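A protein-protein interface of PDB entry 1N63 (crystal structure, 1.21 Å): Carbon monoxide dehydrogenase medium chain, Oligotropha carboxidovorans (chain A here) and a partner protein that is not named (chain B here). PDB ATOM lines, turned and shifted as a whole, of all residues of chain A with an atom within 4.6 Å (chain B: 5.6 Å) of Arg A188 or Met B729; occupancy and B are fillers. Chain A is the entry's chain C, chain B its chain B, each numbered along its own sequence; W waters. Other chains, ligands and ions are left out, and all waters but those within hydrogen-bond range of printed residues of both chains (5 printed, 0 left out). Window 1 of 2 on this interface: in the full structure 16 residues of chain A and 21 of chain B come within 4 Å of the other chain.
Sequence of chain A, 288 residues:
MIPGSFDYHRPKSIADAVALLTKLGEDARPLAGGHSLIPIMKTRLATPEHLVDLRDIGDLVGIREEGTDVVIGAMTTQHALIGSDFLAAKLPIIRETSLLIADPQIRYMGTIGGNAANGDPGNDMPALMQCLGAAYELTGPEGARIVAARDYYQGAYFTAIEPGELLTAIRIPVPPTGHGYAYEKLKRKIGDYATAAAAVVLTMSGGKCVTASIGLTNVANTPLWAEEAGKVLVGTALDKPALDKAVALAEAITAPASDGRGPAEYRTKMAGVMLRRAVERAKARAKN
The side-chain carboxylate (OD1) of Asp B730 is in salt-bridge range of the guanidinium group (NH1) of Arg A188, 2.9 Å away.
The backbone carbonyl oxygen (O) of Met B729 sits at hydrogen-bond distance from the guanidinium group (NH2) of Arg A188, 3.2 Å away.
N of Met B729 lies close to OG of Ser B727, 3.1 Å away.
NE of Arg A188 lies within salt-bridge range of OD2 of Asp A192, at 2.9 Å.
Among the printed residues, merely in contact across the chains: Arg A188 with Phe B732 (3.5 Å) and Lys A189 with Glu B738 (3.3 Å).
Of the printed residues of chain B, Lys A189 touches Glu B738 (3.3 Å).
Of the printed residues of chain A, Met B729 touches Arg A188.
Printed residues of chain A within 4 Å of Asp B730: Arg A188.
Of the printed residues of chain A, Phe B732 touches Arg A188 (3.5 Å).
Of the printed residues of chain A, Glu B738 touches Lys A189.
The nearest printed residue of chain B that does not touch Arg A188 is Glu B738 (4.7 Å).
The nearest printed residue of chain A that does not touch Phe B732 is Lys A189 (4.04 Å).
Of the 6 printed residues of chain A, 2 touch a printed residue of chain B.
Along chain A the printed residues that touch a printed residue of chain B span positions 188 to 189.
Of the 8 printed residues of chain B, 4 touch a printed residue of chain A.
Hydrophobic or aromatic side chains of chain B that line the printed part of chain A: Phe B732.
Water W2 lies within hydrogen-bond range of O of Phe B731 (2.7 Å), O of Phe B728 (2.8 Å) and NZ of Lys A189 (2.8 Å).
Water W1 lies within hydrogen-bond range of NH1 of Arg A188 (2.7 Å), O of Gly A260 (3.3 Å) and O of Asp B730 (3.5 Å).
Water W4 lies within hydrogen-bond range of OD1 of Asp B730 (2.7 Å) and N of Gly A260 (2.8 Å).
Water W5 lies within hydrogen-bond range of OD2 of Asp B794 (2.7 Å) and O of Gly A260 (2.9 Å).
Water W3 lies within hydrogen-bond range of the backbone carbonyl oxygen of Met B729 (2.8 Å), the side-chain carboxylate of Asp A192 (2.9 Å) and the guanidinium group of Arg A261 (3.3 Å).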
ATOM      1  N   LYS A 187      -1.899 -22.954  -9.622  1.00  0.00           N
ATOM      2  CA  LYS A 187      -1.621 -24.153 -10.359  1.00  0.00           C
ATOM      3  C   LYS A 187      -0.392 -23.949 -11.248  1.00  0.00           C
ATOM      4  O   LYS A 187      -0.032 -22.816 -11.498  1.00  0.00           O
ATOM      5  CB  LYS A 187      -2.832 -24.543 -11.207  1.00  0.00           C
ATOM      6  CG  LYS A 187      -3.210 -23.556 -12.277  1.00  0.00           C
ATOM      7  CD  LYS A 187      -4.528 -23.946 -12.922  1.00  0.00           C
ATOM      8  CE  LYS A 187      -4.824 -23.153 -14.145  1.00  0.00           C
ATOM      9  NZ  LYS A 187      -4.863 -21.687 -13.845  1.00  0.00           N
ATOM     10  N   ARG A 188       0.229 -25.017 -11.722  1.00  0.00           N
ATOM     11  CA  ARG A 188       1.440 -24.879 -12.492  1.00  0.00           C
ATOM     12  C   ARG A 188       1.183 -24.438 -13.939  1.00  0.00           C
ATOM     13  O   ARG A 188       2.049 -23.860 -14.553  1.00  0.00           O
ATOM     14  CB  ARG A 188       2.191 -26.211 -12.467  1.00  0.00           C
ATOM     15  CG  ARG A 188       2.860 -26.525 -11.150  1.00  0.00           C
ATOM     16  CD  ARG A 188       3.430 -27.916 -11.066  1.00  0.00           C
ATOM     17  NE  ARG A 188       2.419 -28.937 -11.259  1.00  0.00           N
ATOM     18  CZ  ARG A 188       2.664 -30.236 -11.271  1.00  0.00           C
ATOM     19  NH1 ARG A 188       3.905 -30.711 -11.144  1.00  0.00           N
ATOM     20  NH2 ARG A 188       1.653 -31.067 -11.397  1.00  0.00           N
ATOM     21  N   LYS A 189       0.026 -24.773 -14.494  1.00  0.00           N
ATOM     22  CA  LYS A 189      -0.350 -24.467 -15.872  1.00  0.00           C
ATOM     23  C   LYS A 189      -1.800 -24.846 -16.050  1.00  0.00           C
ATOM     24  O   LYS A 189      -2.378 -25.518 -15.172  1.00  0.00           O
ATOM     25  CB  LYS A 189       0.493 -25.243 -16.898  1.00  0.00           C
ATOM     26  CG  LYS A 189       0.556 -26.749 -16.679  1.00  0.00           C
ATOM     27  CD  LYS A 189       1.277 -27.485 -17.783  1.00  0.00           C
ATOM     28  CE  LYS A 189       0.296 -27.774 -18.878  1.00  0.00           C
ATOM     29  NZ  LYS A 189       0.920 -28.523 -19.997  1.00  0.00           N
ATOM     30  N   ASP A 192      -3.772 -28.202 -14.760  1.00  0.00           N
ATOM     31  CA  ASP A 192      -3.163 -28.803 -13.582  1.00  0.00           C
ATOM     32  C   ASP A 192      -4.103 -28.711 -12.383  1.00  0.00           C
ATOM     33  O   ASP A 192      -4.769 -27.712 -12.168  1.00  0.00           O
ATOM     34  CB  ASP A 192      -1.873 -28.060 -13.310  1.00  0.00           C
ATOM     35  CG  ASP A 192      -1.012 -28.666 -12.233  1.00  0.00           C
ATOM     36  OD1 ASP A 192      -1.030 -29.904 -12.050  1.00  0.00           O
ATOM     37  OD2 ASP A 192      -0.237 -27.911 -11.563  1.00  0.00           O
ATOM     38  N   GLY A 260       5.122 -32.938  -7.179  1.00  0.00           N
ATOM     39  CA  GLY A 260       5.776 -31.998  -8.070  1.00  0.00           C
ATOM     40  C   GLY A 260       5.308 -30.553  -7.887  1.00  0.00           C
ATOM     41  O   GLY A 260       5.996 -29.643  -8.369  1.00  0.00           O
ATOM     42  N   ARG A 261       4.189 -30.344  -7.195  1.00  0.00           N
ATOM     43  CA  ARG A 261       3.736 -29.012  -6.901  1.00  0.00           C
ATOM     44  C   ARG A 261       4.470 -28.331  -5.732  1.00  0.00           C
ATOM     45  O   ARG A 261       4.269 -27.150  -5.436  1.00  0.00           O
ATOM     46  CB  ARG A 261       2.246 -29.073  -6.613  1.00  0.00           C
ATOM     47  CG  ARG A 261       1.453 -29.522  -7.816  1.00  0.00           C
ATOM     48  CD  ARG A 261      -0.023 -29.785  -7.523  1.00  0.00           C
ATOM     49  NE  ARG A 261      -0.739 -30.396  -8.636  1.00  0.00           N
ATOM     50  CZ  ARG A 261      -0.581 -31.669  -9.011  1.00  0.00           C
ATOM     51  NH1 ARG A 261       0.126 -32.528  -8.268  1.00  0.00           N
ATOM     52  NH2 ARG A 261      -1.193 -32.088 -10.098  1.00  0.00           N
ATOM     53  N   SER B 727       5.581 -37.421 -17.297  1.00  0.00           N
ATOM     54  CA  SER B 727       4.328 -37.454 -18.031  1.00  0.00           C
ATOM     55  C   SER B 727       3.815 -36.030 -18.096  1.00  0.00           C
ATOM     56  O   SER B 727       4.248 -35.195 -17.321  1.00  0.00           O
ATOM     57  CB  SER B 727       3.291 -38.325 -17.336  1.00  0.00           C
ATOM     58  OG  SER B 727       2.611 -37.631 -16.291  1.00  0.00           O
ATOM     59  N   PHE B 728       2.844 -35.793 -18.959  1.00  0.00           N
ATOM     60  CA  PHE B 728       2.307 -34.454 -19.057  1.00  0.00           C
ATOM     61  C   PHE B 728       1.421 -34.051 -17.866  1.00  0.00           C
ATOM     62  O   PHE B 728       0.995 -32.904 -17.772  1.00  0.00           O
ATOM     63  CB  PHE B 728       1.577 -34.276 -20.395  1.00  0.00           C
ATOM     64  CG  PHE B 728       2.468 -34.249 -21.621  1.00  0.00           C
ATOM     65  CD1 PHE B 728       3.859 -34.152 -21.587  1.00  0.00           C
ATOM     66  CD2 PHE B 728       1.874 -34.314 -22.865  1.00  0.00           C
ATOM     67  CE1 PHE B 728       4.613 -34.075 -22.757  1.00  0.00           C
ATOM     68  CE2 PHE B 728       2.628 -34.240 -24.010  1.00  0.00           C
ATOM     69  CZ  PHE B 728       3.987 -34.154 -23.941  1.00  0.00           C
ATOM     70  N   MET B 729       1.243 -34.945 -16.893  1.00  0.00           N
ATOM     71  CA  MET B 729       0.662 -34.515 -15.625  1.00  0.00           C
ATOM     72  C   MET B 729       1.584 -33.531 -14.864  1.00  0.00           C
ATOM     73  O   MET B 729       1.090 -32.666 -14.129  1.00  0.00           O
ATOM     74  CB  MET B 729       0.310 -35.722 -14.779  1.00  0.00           C
ATOM     75  CG  MET B 729      -0.948 -36.476 -15.236  1.00  0.00           C
ATOM     76  SD  MET B 729      -1.197 -38.007 -14.295  1.00  0.00           S
ATOM     77  N   ASP B 730       2.888 -33.622 -15.067  1.00  0.00           N
ATOM     78  CA  ASP B 730       3.826 -32.791 -14.323  1.00  0.00           C
ATOM     79  C   ASP B 730       4.835 -32.104 -15.208  1.00  0.00           C
ATOM     80  O   ASP B 730       5.346 -31.069 -14.785  1.00  0.00           O
ATOM     81  CB  ASP B 730       4.634 -33.655 -13.338  1.00  0.00           C
ATOM     82  CG  ASP B 730       3.761 -34.257 -12.294  1.00  0.00           C
ATOM     83  OD1 ASP B 730       3.326 -33.499 -11.390  1.00  0.00           O
ATOM     84  OD2 ASP B 730       3.434 -35.463 -12.305  1.00  0.00           O
ATOM     85  N   PHE B 731       5.218 -32.687 -16.338  1.00  0.00           N
ATOM     86  CA  PHE B 731       6.293 -32.159 -17.185  1.00  0.00           C
ATOM     87  C   PHE B 731       5.786 -30.844 -17.822  1.00  0.00           C
ATOM     88  O   PHE B 731       4.807 -30.867 -18.551  1.00  0.00           O
ATOM     89  CB  PHE B 731       6.610 -33.165 -18.261  1.00  0.00           C
ATOM     90  CG  PHE B 731       7.780 -32.797 -19.121  1.00  0.00           C
ATOM     91  CD1 PHE B 731       9.071 -32.911 -18.665  1.00  0.00           C
ATOM     92  CD2 PHE B 731       7.577 -32.392 -20.431  1.00  0.00           C
ATOM     93  CE1 PHE B 731      10.116 -32.641 -19.504  1.00  0.00           C
ATOM     94  CE2 PHE B 731       8.622 -32.077 -21.249  1.00  0.00           C
ATOM     95  CZ  PHE B 731       9.879 -32.134 -20.762  1.00  0.00           C
ATOM     96  N   PHE B 732       6.425 -29.722 -17.507  1.00  0.00           N
ATOM     97  CA  PHE B 732       5.909 -28.416 -17.878  1.00  0.00           C
ATOM     98  C   PHE B 732       6.097 -28.161 -19.378  1.00  0.00           C
ATOM     99  O   PHE B 732       7.153 -27.810 -19.850  1.00  0.00           O
ATOM    100  CB  PHE B 732       6.603 -27.334 -17.044  1.00  0.00           C
ATOM    101  CG  PHE B 732       6.084 -25.944 -17.306  1.00  0.00           C
ATOM    102  CD1 PHE B 732       4.815 -25.559 -16.898  1.00  0.00           C
ATOM    103  CD2 PHE B 732       6.915 -25.017 -17.895  1.00  0.00           C
ATOM    104  CE1 PHE B 732       4.406 -24.240 -17.063  1.00  0.00           C
ATOM    105  CE2 PHE B 732       6.455 -23.731 -18.072  1.00  0.00           C
ATOM    106  CZ  PHE B 732       5.187 -23.382 -17.712  1.00  0.00           C
ATOM    107  N   GLU B 738       0.243 -19.729 -20.901  1.00  0.00           N
ATOM    108  CA  GLU B 738       1.495 -19.464 -20.185  1.00  0.00           C
ATOM    109  C   GLU B 738       2.546 -18.803 -21.072  1.00  0.00           C
ATOM    110  O   GLU B 738       3.467 -18.156 -20.550  1.00  0.00           O
ATOM    111  CB  GLU B 738       2.097 -20.733 -19.565  1.00  0.00           C
ATOM    112  CG  GLU B 738       1.236 -21.368 -18.476  1.00  0.00           C
ATOM    113  CD  GLU B 738       0.075 -22.165 -19.030  1.00  0.00           C
ATOM    114  OE1 GLU B 738       0.194 -22.769 -20.104  1.00  0.00           O
ATOM    115  OE2 GLU B 738      -0.940 -22.266 -18.317  1.00  0.00           O
ATOM    116  N   ASP B 794      10.295 -22.416 -10.842  1.00  0.00           N
ATOM    117  CA  ASP B 794       8.864 -22.572 -10.653  1.00  0.00           C
ATOM    118  C   ASP B 794       8.497 -22.030  -9.268  1.00  0.00           C
ATOM    119  O   ASP B 794       9.353 -21.592  -8.489  1.00  0.00           O
ATOM    120  CB  ASP B 794       8.425 -24.029 -10.913  1.00  0.00           C
ATOM    121  CG  ASP B 794       8.979 -25.035  -9.938  1.00  0.00           C
ATOM    122  OD1 ASP B 794       9.794 -24.662  -9.052  1.00  0.00           O
ATOM    123  OD2 ASP B 794       8.605 -26.243 -10.025  1.00  0.00           O
HETATM  124  O   HOH W   1       6.390 -29.883 -11.673  1.00  0.00           O
HETATM  125  O   HOH W   2       2.251 -30.884 -19.259  1.00  0.00           O
HETATM  126  O   HOH W   3      -1.577 -32.377 -13.413  1.00  0.00           O
HETATM  127  O   HOH W   4       3.598 -34.606  -8.915  1.00  0.00           O
HETATM  128  O   HOH W   5       6.024 -26.954  -9.407  1.00  0.00           O
